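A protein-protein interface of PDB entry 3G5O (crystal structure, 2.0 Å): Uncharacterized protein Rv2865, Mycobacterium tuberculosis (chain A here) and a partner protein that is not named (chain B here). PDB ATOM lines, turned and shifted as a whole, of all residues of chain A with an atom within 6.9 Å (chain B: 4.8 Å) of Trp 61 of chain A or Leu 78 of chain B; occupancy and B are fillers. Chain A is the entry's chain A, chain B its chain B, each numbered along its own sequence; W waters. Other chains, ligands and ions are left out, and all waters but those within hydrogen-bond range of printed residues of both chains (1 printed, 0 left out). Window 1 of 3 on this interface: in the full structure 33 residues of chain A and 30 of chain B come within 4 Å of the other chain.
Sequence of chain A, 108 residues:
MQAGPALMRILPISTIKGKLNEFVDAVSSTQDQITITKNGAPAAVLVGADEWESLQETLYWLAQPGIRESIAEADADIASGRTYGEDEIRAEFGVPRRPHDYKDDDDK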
ATOM      1  N   GLN A  56       4.537   7.175   0.606  1.00  0.00           N
ATOM      2  CA  GLN A  56       3.919   6.931   1.918  1.00  0.00           C
ATOM      3  C   GLN A  56       3.854   5.435   2.258  1.00  0.00           C
ATOM      4  O   GLN A  56       4.111   5.054   3.381  1.00  0.00           O
ATOM      5  CB  GLN A  56       2.491   7.525   2.007  1.00  0.00           C
ATOM      6  CG  GLN A  56       2.437   9.098   1.842  1.00  0.00           C
ATOM      7  CD  GLN A  56       3.463   9.782   2.746  1.00  0.00           C
ATOM      8  OE1 GLN A  56       3.519   9.519   3.942  1.00  0.00           O
ATOM      9  NE2 GLN A  56       4.301  10.614   2.170  1.00  0.00           N
ATOM     10  N   GLU A  57       3.492   4.581   1.287  1.00  0.00           N
ATOM     11  CA  GLU A  57       3.416   3.164   1.569  1.00  0.00           C
ATOM     12  C   GLU A  57       4.822   2.543   1.702  1.00  0.00           C
ATOM     13  O   GLU A  57       5.021   1.592   2.459  1.00  0.00           O
ATOM     14  CB  GLU A  57       2.585   2.448   0.479  1.00  0.00           C
ATOM     15  CG  GLU A  57       1.126   2.817   0.500  1.00  0.00           C
ATOM     16  CD  GLU A  57       0.526   2.491   1.879  1.00  0.00           C
ATOM     17  OE1 GLU A  57       0.432   1.281   2.216  1.00  0.00           O
ATOM     18  OE2 GLU A  57       0.247   3.442   2.652  1.00  0.00           O
ATOM     19  N   THR A  58       5.807   3.061   0.963  1.00  0.00           N
ATOM     20  CA  THR A  58       7.158   2.565   1.129  1.00  0.00           C
ATOM     21  C   THR A  58       7.662   2.860   2.549  1.00  0.00           C
ATOM     22  O   THR A  58       8.293   2.007   3.194  1.00  0.00           O
ATOM     23  CB  THR A  58       8.115   3.199   0.089  1.00  0.00           C
ATOM     24  OG1 THR A  58       7.622   2.910  -1.220  1.00  0.00           O
ATOM     25  CG2 THR A  58       9.515   2.638   0.234  1.00  0.00           C
ATOM     26  N   LEU A  59       7.417   4.087   2.992  1.00  0.00           N
ATOM     27  CA  LEU A  59       7.739   4.501   4.365  1.00  0.00           C
ATOM     28  C   LEU A  59       7.083   3.580   5.383  1.00  0.00           C
ATOM     29  O   LEU A  59       7.745   3.084   6.307  1.00  0.00           O
ATOM     30  CB  LEU A  59       7.271   5.928   4.634  1.00  0.00           C
ATOM     31  CG  LEU A  59       8.075   7.087   4.058  1.00  0.00           C
ATOM     32  CD1 LEU A  59       7.156   8.272   4.216  1.00  0.00           C
ATOM     33  CD2 LEU A  59       9.380   7.300   4.837  1.00  0.00           C
ATOM     34  N   TYR A  60       5.791   3.317   5.208  1.00  0.00           N
ATOM     35  CA  TYR A  60       5.128   2.402   6.123  1.00  0.00           C
ATOM     36  C   TYR A  60       5.839   1.030   6.190  1.00  0.00           C
ATOM     37  O   TYR A  60       6.197   0.541   7.284  1.00  0.00           O
ATOM     38  CB  TYR A  60       3.645   2.183   5.734  1.00  0.00           C
ATOM     39  CG  TYR A  60       3.061   1.110   6.641  1.00  0.00           C
ATOM     40  CD1 TYR A  60       2.569   1.436   7.909  1.00  0.00           C
ATOM     41  CD2 TYR A  60       3.043  -0.223   6.249  1.00  0.00           C
ATOM     42  CE1 TYR A  60       2.073   0.439   8.777  1.00  0.00           C
ATOM     43  CE2 TYR A  60       2.545  -1.205   7.084  1.00  0.00           C
ATOM     44  CZ  TYR A  60       2.073  -0.869   8.350  1.00  0.00           C
ATOM     45  OH  TYR A  60       1.589  -1.864   9.171  1.00  0.00           O
ATOM     46  N   TRP A  61       5.992   0.406   5.020  1.00  0.00           N
ATOM     47  CA  TRP A  61       6.457  -0.989   4.985  1.00  0.00           C
ATOM     48  C   TRP A  61       7.890  -1.173   5.464  1.00  0.00           C
ATOM     49  O   TRP A  61       8.181  -2.161   6.187  1.00  0.00           O
ATOM     50  CB  TRP A  61       6.255  -1.630   3.622  1.00  0.00           C
ATOM     51  CG  TRP A  61       4.823  -2.062   3.437  1.00  0.00           C
ATOM     52  CD1 TRP A  61       3.880  -1.485   2.631  1.00  0.00           C
ATOM     53  CD2 TRP A  61       4.184  -3.171   4.084  1.00  0.00           C
ATOM     54  NE1 TRP A  61       2.692  -2.182   2.721  1.00  0.00           N
ATOM     55  CE2 TRP A  61       2.844  -3.214   3.615  1.00  0.00           C
ATOM     56  CE3 TRP A  61       4.607  -4.109   5.031  1.00  0.00           C
ATOM     57  CZ2 TRP A  61       1.920  -4.173   4.052  1.00  0.00           C
ATOM     58  CZ3 TRP A  61       3.683  -5.088   5.471  1.00  0.00           C
ATOM     59  CH2 TRP A  61       2.355  -5.096   4.980  1.00  0.00           C
ATOM     60  N   LEU A  62       8.767  -0.211   5.106  1.00  0.00           N
ATOM     61  CA  LEU A  62      10.183  -0.284   5.558  1.00  0.00           C
ATOM     62  C   LEU A  62      10.329  -0.218   7.078  1.00  0.00           C
ATOM     63  O   LEU A  62      11.338  -0.670   7.618  1.00  0.00           O
ATOM     64  CB  LEU A  62      11.047   0.835   4.900  1.00  0.00           C
ATOM     65  CG  LEU A  62      11.318   0.637   3.401  1.00  0.00           C
ATOM     66  CD1 LEU A  62      12.110   1.789   2.840  1.00  0.00           C
ATOM     67  CD2 LEU A  62      12.074  -0.660   3.163  1.00  0.00           C
ATOM     68  N   ALA A  63       9.325   0.364   7.750  1.00  0.00           N
ATOM     69  CA  ALA A  63       9.307   0.490   9.223  1.00  0.00           C
ATOM     70  C   ALA A  63       8.775  -0.746   9.973  1.00  0.00           C
ATOM     71  O   ALA A  63       8.757  -0.746  11.219  1.00  0.00           O
ATOM     72  CB  ALA A  63       8.503   1.749   9.645  1.00  0.00           C
ATOM     73  N   GLN A  64       8.320  -1.777   9.235  1.00  0.00           N
ATOM     74  CA  GLN A  64       7.749  -2.952   9.898  1.00  0.00           C
ATOM     75  C   GLN A  64       8.821  -3.998  10.306  1.00  0.00           C
ATOM     76  O   GLN A  64       9.798  -4.211   9.592  1.00  0.00           O
ATOM     77  CB  GLN A  64       6.646  -3.584   9.043  1.00  0.00           C
ATOM     78  CG  GLN A  64       5.563  -2.585   8.676  1.00  0.00           C
ATOM     79  CD  GLN A  64       5.048  -1.795   9.895  1.00  0.00           C
ATOM     80  OE1 GLN A  64       4.646  -2.392  10.890  1.00  0.00           O
ATOM     81  NE2 GLN A  64       5.042  -0.454   9.799  1.00  0.00           N
ATOM     82  N   PRO A  65       8.644  -4.629  11.475  1.00  0.00           N
ATOM     83  CA  PRO A  65       9.674  -5.562  11.961  1.00  0.00           C
ATOM     84  C   PRO A  65       9.788  -6.778  11.053  1.00  0.00           C
ATOM     85  O   PRO A  65       8.745  -7.306  10.602  1.00  0.00           O
ATOM     86  CB  PRO A  65       9.169  -6.008  13.358  1.00  0.00           C
ATOM     87  CG  PRO A  65       7.727  -5.622  13.445  1.00  0.00           C
ATOM     88  CD  PRO A  65       7.458  -4.527  12.368  1.00  0.00           C
ATOM     89  N   ILE A  67      10.571  -7.014   8.043  1.00  0.00           N
ATOM     90  CA  ILE A  67      10.029  -6.815   6.672  1.00  0.00           C
ATOM     91  C   ILE A  67      10.859  -7.517   5.588  1.00  0.00           C
ATOM     92  O   ILE A  67      10.299  -8.240   4.753  1.00  0.00           O
ATOM     93  CB  ILE A  67       9.688  -5.287   6.311  1.00  0.00           C
ATOM     94  CG1 ILE A  67       8.953  -5.205   4.956  1.00  0.00           C
ATOM     95  CG2 ILE A  67      10.939  -4.417   6.300  1.00  0.00           C
ATOM     96  CD1 ILE A  67       7.656  -6.053   4.936  1.00  0.00           C
ATOM     97  N   ARG A  68      12.185  -7.357   5.597  1.00  0.00           N
ATOM     98  CA  ARG A  68      12.987  -7.940   4.514  1.00  0.00           C
ATOM     99  C   ARG A  68      13.004  -9.489   4.537  1.00  0.00           C
ATOM    100  O   ARG A  68      12.941 -10.137   3.466  1.00  0.00           O
ATOM    101  CB  ARG A  68      14.416  -7.383   4.540  1.00  0.00           C
ATOM    102  CG  ARG A  68      14.486  -5.901   4.202  1.00  0.00           C
ATOM    103  CD  ARG A  68      15.804  -5.288   4.751  1.00  0.00           C
ATOM    104  NE  ARG A  68      15.869  -3.847   4.467  1.00  0.00           N
ATOM    105  CZ  ARG A  68      15.354  -2.916   5.249  1.00  0.00           C
ATOM    106  NH1 ARG A  68      14.728  -3.269   6.362  1.00  0.00           N
ATOM    107  NH2 ARG A  68      15.466  -1.629   4.912  1.00  0.00           N
ATOM    108  N   SER A  70      10.560 -11.335   5.902  1.00  0.00           N
ATOM    109  CA  SER A  70       9.212 -11.651   5.426  1.00  0.00           C
ATOM    110  C   SER A  70       9.171 -11.808   3.918  1.00  0.00           C
ATOM    111  O   SER A  70       8.596 -12.767   3.398  1.00  0.00           O
ATOM    112  CB  SER A  70       8.217 -10.510   5.756  1.00  0.00           C
ATOM    113  OG  SER A  70       7.636 -10.727   7.012  1.00  0.00           O
ATOM    114  N   ILE A  71       9.715 -10.816   3.225  1.00  0.00           N
ATOM    115  CA  ILE A  71       9.679 -10.792   1.765  1.00  0.00           C
ATOM    116  C   ILE A  71      10.525 -11.918   1.171  1.00  0.00           C
ATOM    117  O   ILE A  71      10.104 -12.581   0.238  1.00  0.00           O
ATOM    118  CB  ILE A  71      10.123  -9.431   1.227  1.00  0.00           C
ATOM    119  CG1 ILE A  71       9.069  -8.363   1.557  1.00  0.00           C
ATOM    120  CG2 ILE A  71      10.289  -9.461  -0.272  1.00  0.00           C
ATOM    121  CD1 ILE A  71       9.647  -6.978   1.468  1.00  0.00           C
ATOM    122  N   LEU B  60       5.686  -0.021  -4.741  1.00  0.00           N
ATOM    123  CA  LEU B  60       6.587   0.515  -3.749  1.00  0.00           C
ATOM    124  C   LEU B  60       7.948   0.852  -4.362  1.00  0.00           C
ATOM    125  O   LEU B  60       8.256   0.465  -5.504  1.00  0.00           O
ATOM    126  CB  LEU B  60       6.710  -0.458  -2.554  1.00  0.00           C
ATOM    127  CG  LEU B  60       5.373  -0.824  -1.915  1.00  0.00           C
ATOM    128  CD1 LEU B  60       5.593  -1.610  -0.596  1.00  0.00           C
ATOM    129  CD2 LEU B  60       4.573   0.498  -1.652  1.00  0.00           C
ATOM    130  N   LEU B  64      12.109  -1.868  -1.896  1.00  0.00           N
ATOM    131  CA  LEU B  64      10.823  -2.589  -2.038  1.00  0.00           C
ATOM    132  C   LEU B  64      10.288  -2.570  -3.471  1.00  0.00           C
ATOM    133  O   LEU B  64       9.170  -3.028  -3.727  1.00  0.00           O
ATOM    134  CB  LEU B  64       9.776  -1.995  -1.071  1.00  0.00           C
ATOM    135  CG  LEU B  64      10.098  -2.115   0.437  1.00  0.00           C
ATOM    136  CD1 LEU B  64       8.917  -1.664   1.282  1.00  0.00           C
ATOM    137  CD2 LEU B  64      10.458  -3.503   0.825  1.00  0.00           C
ATOM    138  N   THR B  67       7.176  -4.692  -5.477  1.00  0.00           N
ATOM    139  CA  THR B  67       6.045  -5.075  -4.644  1.00  0.00           C
ATOM    140  C   THR B  67       5.052  -3.915  -4.626  1.00  0.00           C
ATOM    141  O   THR B  67       5.387  -2.791  -5.083  1.00  0.00           O
ATOM    142  CB  THR B  67       6.478  -5.438  -3.205  1.00  0.00           C
ATOM    143  OG1 THR B  67       6.921  -4.258  -2.505  1.00  0.00           O
ATOM    144  CG2 THR B  67       7.615  -6.480  -3.205  1.00  0.00           C
ATOM    145  N   PHE B  68       3.845  -4.174  -4.102  1.00  0.00           N
ATOM    146  CA  PHE B  68       2.731  -3.227  -4.190  1.00  0.00           C
ATOM    147  C   PHE B  68       2.098  -3.259  -2.827  1.00  0.00           C
ATOM    148  O   PHE B  68       2.128  -4.305  -2.177  1.00  0.00           O
ATOM    149  CB  PHE B  68       1.665  -3.708  -5.187  1.00  0.00           C
ATOM    150  CG  PHE B  68       2.021  -3.471  -6.605  1.00  0.00           C
ATOM    151  CD1 PHE B  68       1.511  -2.362  -7.282  1.00  0.00           C
ATOM    152  CD2 PHE B  68       2.908  -4.342  -7.273  1.00  0.00           C
ATOM    153  CE1 PHE B  68       1.888  -2.108  -8.638  1.00  0.00           C
ATOM    154  CE2 PHE B  68       3.269  -4.109  -8.633  1.00  0.00           C
ATOM    155  CZ  PHE B  68       2.765  -2.987  -9.300  1.00  0.00           C
ATOM    156  N   SER B  69       1.508  -2.151  -2.395  1.00  0.00           N
ATOM    157  CA  SER B  69       0.795  -2.124  -1.114  1.00  0.00           C
ATOM    158  C   SER B  69      -0.614  -1.691  -1.377  1.00  0.00           C
ATOM    159  O   SER B  69      -0.817  -0.663  -2.004  1.00  0.00           O
ATOM    160  CB  SER B  69       1.413  -1.110  -0.114  1.00  0.00           C
ATOM    161  OG  SER B  69       0.695  -1.077   1.153  1.00  0.00           O
ATOM    162  N   ARG B  76      -3.328  -3.711   5.704  1.00  0.00           N
ATOM    163  CA  ARG B  76      -2.573  -3.454   4.473  1.00  0.00           C
ATOM    164  C   ARG B  76      -2.160  -4.802   3.917  1.00  0.00           C
ATOM    165  O   ARG B  76      -1.893  -5.736   4.688  1.00  0.00           O
ATOM    166  CB  ARG B  76      -1.350  -2.629   4.780  1.00  0.00           C
ATOM    167  CG  ARG B  76      -1.577  -1.099   4.829  1.00  0.00           C
ATOM    168  CD  ARG B  76      -0.198  -0.444   5.035  1.00  0.00           C
ATOM    169  NE  ARG B  76      -0.185   0.996   4.904  1.00  0.00           N
ATOM    170  CZ  ARG B  76      -0.421   1.858   5.888  1.00  0.00           C
ATOM    171  NH1 ARG B  76      -0.724   1.458   7.141  1.00  0.00           N
ATOM    172  NH2 ARG B  76      -0.363   3.134   5.608  1.00  0.00           N
ATOM    173  N   LEU B  77      -2.140  -4.932   2.587  1.00  0.00           N
ATOM    174  CA  LEU B  77      -1.602  -6.161   1.977  1.00  0.00           C
ATOM    175  C   LEU B  77      -0.371  -5.788   1.171  1.00  0.00           C
ATOM    176  O   LEU B  77      -0.386  -4.766   0.473  1.00  0.00           O
ATOM    177  CB  LEU B  77      -2.637  -6.773   1.011  1.00  0.00           C
ATOM    178  CG  LEU B  77      -4.071  -7.076   1.450  1.00  0.00           C
ATOM    179  CD1 LEU B  77      -4.716  -7.985   0.402  1.00  0.00           C
ATOM    180  CD2 LEU B  77      -4.099  -7.774   2.772  1.00  0.00           C
ATOM    181  N   LEU B  78       0.655  -6.625   1.238  1.00  0.00           N
ATOM    182  CA  LEU B  78       1.863  -6.429   0.478  1.00  0.00           C
ATOM    183  C   LEU B  78       1.843  -7.552  -0.546  1.00  0.00           C
ATOM    184  O   LEU B  78       1.638  -8.728  -0.173  1.00  0.00           O
ATOM    185  CB  LEU B  78       3.097  -6.543   1.378  1.00  0.00           C
ATOM    186  CG  LEU B  78       4.449  -6.355   0.659  1.00  0.00           C
ATOM    187  CD1 LEU B  78       4.561  -4.875   0.200  1.00  0.00           C
ATOM    188  CD2 LEU B  78       5.601  -6.773   1.612  1.00  0.00           C
ATOM    189  N   TYR B  79       2.030  -7.207  -1.819  1.00  0.00           N
ATOM    190  CA  TYR B  79       1.856  -8.202  -2.875  1.00  0.00           C
ATOM    191  C   TYR B  79       2.715  -7.982  -4.114  1.00  0.00           C
ATOM    192  O   TYR B  79       3.341  -6.932  -4.270  1.00  0.00           O
ATOM    193  CB  TYR B  79       0.379  -8.389  -3.244  1.00  0.00           C
ATOM    194  CG  TYR B  79      -0.320  -7.154  -3.799  1.00  0.00           C
ATOM    195  CD1 TYR B  79      -0.529  -7.005  -5.165  1.00  0.00           C
ATOM    196  CD2 TYR B  79      -0.736  -6.127  -2.946  1.00  0.00           C
ATOM    197  CE1 TYR B  79      -1.170  -5.869  -5.687  1.00  0.00           C
ATOM    198  CE2 TYR B  79      -1.418  -4.995  -3.437  1.00  0.00           C
ATOM    199  CZ  TYR B  79      -1.630  -4.867  -4.803  1.00  0.00           C
ATOM    200  OH  TYR B  79      -2.299  -3.749  -5.283  1.00  0.00           O
ATOM    201  N   ARG B  80       2.792  -9.010  -4.949  1.00  0.00           N
ATOM    202  CA  ARG B  80       3.389  -8.873  -6.272  1.00  0.00           C
ATOM    203  C   ARG B  80       2.314  -9.106  -7.329  1.00  0.00           C
ATOM    204  O   ARG B  80       1.293  -9.770  -7.077  1.00  0.00           O
ATOM    205  CB  ARG B  80       4.541  -9.865  -6.468  1.00  0.00           C
ATOM    206  CG  ARG B  80       5.773  -9.538  -5.672  1.00  0.00           C
ATOM    207  CD  ARG B  80       6.905 -10.589  -5.894  1.00  0.00           C
ATOM    208  NE  ARG B  80       8.014 -10.446  -4.948  1.00  0.00           N
ATOM    209  CZ  ARG B  80       8.947  -9.482  -4.990  1.00  0.00           C
ATOM    210  NH1 ARG B  80       8.940  -8.524  -5.935  1.00  0.00           N
ATOM    211  NH2 ARG B  80       9.908  -9.475  -4.091  1.00  0.00           N
ATOM    212  N   VAL B  89       0.074 -12.252  -5.981  1.00  0.00           N
ATOM    213  CA  VAL B  89       0.500 -13.103  -4.876  1.00  0.00           C
ATOM    214  C   VAL B  89       0.728 -12.250  -3.637  1.00  0.00           C
ATOM    215  O   VAL B  89       1.490 -11.289  -3.693  1.00  0.00           O
ATOM    216  CB  VAL B  89       1.806 -13.910  -5.214  1.00  0.00           C
ATOM    217  CG1 VAL B  89       2.157 -14.823  -4.064  1.00  0.00           C
ATOM    218  CG2 VAL B  89       1.626 -14.745  -6.458  1.00  0.00           C
ATOM    219  N   ILE B  90       0.069 -12.608  -2.526  1.00  0.00           N
ATOM    220  CA  ILE B  90       0.127 -11.832  -1.280  1.00  0.00           C
ATOM    221  C   ILE B  90       1.341 -12.305  -0.496  1.00  0.00           C
ATOM    222  O   ILE B  90       1.501 -13.498  -0.267  1.00  0.00           O
ATOM    223  CB  ILE B  90      -1.164 -12.010  -0.406  1.00  0.00           C
ATOM    224  CG1 ILE B  90      -2.426 -11.789  -1.238  1.00  0.00           C
ATOM    225  CG2 ILE B  90      -1.165 -11.049   0.804  1.00  0.00           C
ATOM    226  CD1 ILE B  90      -2.409 -10.513  -2.000  1.00  0.00           C
ATOM    227  N   LEU B  91       2.191 -11.371  -0.109  1.00  0.00           N
ATOM    228  CA  LEU B  91       3.381 -11.645   0.669  1.00  0.00           C
ATOM    229  C   LEU B  91       3.178 -11.468   2.180  1.00  0.00           C
ATOM    230  O   LEU B  91       3.716 -12.237   2.980  1.00  0.00           O
ATOM    231  CB  LEU B  91       4.491 -10.711   0.192  1.00  0.00           C
ATOM    232  CG  LEU B  91       4.828 -10.610  -1.311  1.00  0.00           C
ATOM    233  CD1 LEU B  91       6.079  -9.736  -1.464  1.00  0.00           C
ATOM    234  CD2 LEU B  91       5.031 -11.991  -2.041  1.00  0.00           C
ATOM    235  N   ARG B  92       2.398 -10.462   2.568  1.00  0.00           N
ATOM    236  CA  ARG B  92       2.245 -10.113   3.978  1.00  0.00           C
ATOM    237  C   ARG B  92       0.919  -9.405   4.185  1.00  0.00           C
ATOM    238  O   ARG B  92       0.437  -8.708   3.279  1.00  0.00           O
ATOM    239  CB  ARG B  92       3.416  -9.230   4.450  1.00  0.00           C
ATOM    240  CG  ARG B  92       3.414  -8.915   5.993  1.00  0.00           C
ATOM    241  CD  ARG B  92       4.866  -8.666   6.544  1.00  0.00           C
ATOM    242  NE  ARG B  92       4.841  -7.918   7.811  1.00  0.00           N
ATOM    243  CZ  ARG B  92       5.887  -7.736   8.634  1.00  0.00           C
ATOM    244  NH1 ARG B  92       7.082  -8.260   8.356  1.00  0.00           N
ATOM    245  NH2 ARG B  92       5.733  -7.042   9.758  1.00  0.00           N
ATOM    246  N   ASP B  94      -0.755  -6.991   7.181  1.00  0.00           N
ATOM    247  CA  ASP B  94      -0.541  -6.252   8.436  1.00  0.00           C
ATOM    248  C   ASP B  94      -1.857  -5.671   8.942  1.00  0.00           C
ATOM    249  O   ASP B  94      -2.659  -5.194   8.157  1.00  0.00           O
ATOM    250  CB  ASP B  94       0.428  -5.106   8.207  1.00  0.00           C
ATOM    251  CG  ASP B  94       1.846  -5.470   8.539  1.00  0.00           C
ATOM    252  OD1 ASP B  94       2.597  -4.536   8.918  1.00  0.00           O
ATOM    253  OD2 ASP B  94       2.215  -6.682   8.413  1.00  0.00           O
HETATM  254  O   HOH W   1       3.993  -4.908  10.997  1.00  0.00           O
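The guanidinium group of Arg 92 of chain B is in hydrogen-bond range of the side-chain hydroxyl of Ser 70 of chain A (2.9 Å). The side-chain hydroxyl (OG) of Ser 69 of chain B is in hydrogen-bond range of the indole nitrogen (NE1) of Trp 61 of chain A (2.8 Å). The side-chain carboxylate of Glu 57 of chain A lies within hydrogen-bond range of the side-chain hydroxyl of Ser 69 of chain B, 2.6 Å away. The guanidinium group of Arg 76 of chain B lies within salt-bridge range of the side-chain carboxylate of Glu 57 of chain A (2.8 Å). The backbone carbonyl oxygen (O) of Pro 65 of chain A lies within hydrogen-bond range of the guanidinium group (NH1) of Arg 92 of chain B, at 3.0 Å. The side-chain hydroxyl (OH) of Tyr 60 of chain A lies within hydrogen-bond range of the side-chain carboxylate (OD1) of Asp 94 of chain B.
Of the printed residues of chain B, Thr 58 of chain A touches Leu 60 (3.6 Å). Of the printed residues of chain B, Trp 61 of chain A touches Leu 60 (3.7 Å), Leu 64 (3.5 Å), Ser 69 (2.8 Å), Arg 76 (3.7 Å), Leu 78 (3.8 Å), Arg 92 (3.9 Å) and Asp 94 (3.6 Å). Of the printed residues of chain B, Leu 62 of chain A touches Leu 64. Of the printed residues of chain B, Ile 71 of chain A touches Leu 64 (3.6 Å), Leu 78 (3.8 Å) and Arg 80 (3.8 Å). Of the printed residues of chain A, Ser 69 of chain B touches Glu 57 and Trp 61. Leu 77 of chain B touches none of the printed residues of chain A. Of chain A, only Trp 61 (3.8 Å), Ile 67 (3.97 Å) and Ile 71 (3.8 Å) come within 4 Å of Leu 78 of chain B. Tyr 79 of chain B touches none of the printed residues of chain A. Of the printed residues of chain A, Arg 92 of chain B touches Trp 61 (3.9 Å), Gln 64 (3.6 Å), Pro 65 (3.0 Å), Ile 67 (3.7 Å) and Ser 70 (2.9 Å). The nearest printed residue of chain B that does not touch Trp 61 of chain A is Leu 77 of chain B (4.02 Å). The nearest residue of chain A that does not touch Leu 78 of chain B is Ser 70 of chain A (6.2 Å). The nearest printed residue of chain A that does not touch Leu 60 of chain B is Gln 56 of chain A (6.3 Å).
Hydrophobic or aromatic side chains of chain B within 4 Å of the printed part of chain A: Leu 60, Leu 64 and Leu 78. Of the 14 printed residues of chain A, 10 touch a printed residue of chain B. Hydrophobic or aromatic side chains of chain A that line the printed part of chain B: Tyr 60, Trp 61, Leu 62, Ile 67 and Ile 71.
Among the printed residues, pairs that only touch across the chains: Tyr 60 of chain A with Arg 76 of chain B, Glu 57 of chain A with Leu 60 of chain B, Trp 61 of chain A with Leu 64 of chain B, Gln 64 of chain A with Asp 94 of chain B, Trp 61 of chain A with Asp 94 of chain B, Ile 71 of chain A with Leu 64 of chain B, Thr 58 of chain A with Leu 60 of chain B, Gln 64 of chain A with Arg 92 of chain B, Trp 61 of chain A with Leu 60 of chain B, Leu 62 of chain A with Leu 64 of chain B, Trp 61 of chain A with Arg 76 of chain B, Ile 67 of chain A with Arg 92 of chain B, Trp 61 of chain A with Leu 78 of chain B, Ile 71 of chain A with Leu 78 of chain B, Ile 71 of chain A with Arg 80 of chain B, Trp 61 of chain A with Arg 92 of chain B and Ile 67 of chain A with Leu 78 of chain B.
The backbone NH (N) of Leu 78 of chain B sits at hydrogen-bond distance from the backbone carbonyl oxygen (O) of Arg 92 of chain B (2.9 Å). The side-chain amide nitrogen of Gln 64 of chain A is in hydrogen-bond range of the backbone carbonyl oxygen of Tyr 60 of chain A, at 2.9 Å. The backbone carbonyl oxygen (O) of Leu 64 of chain B sits at hydrogen-bond distance from the side-chain hydroxyl (OG1) of Thr 67 of chain B, at 2.8 Å. O of Leu 78 of chain B sits at hydrogen-bond distance from N of Leu 91 of chain B, 2.7 Å away. The backbone NH of Arg 80 of chain B is in hydrogen-bond range of the backbone carbonyl oxygen of Val 89 of chain B, 2.9 Å away. The backbone NH (N) of Leu 60 of chain B sits at hydrogen-bond distance from the backbone carbonyl oxygen (O) of Thr 67 of chain B.
Water W1 lies within hydrogen-bond range of the side-chain carboxylate (OD1) of Asp 94 of chain B (2.5 Å), the side-chain amide oxygen (OE1) of Gln 64 of chain A (2.6 Å) and the guanidinium group (NH2) of Arg 92 of chain B (3.0 Å).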
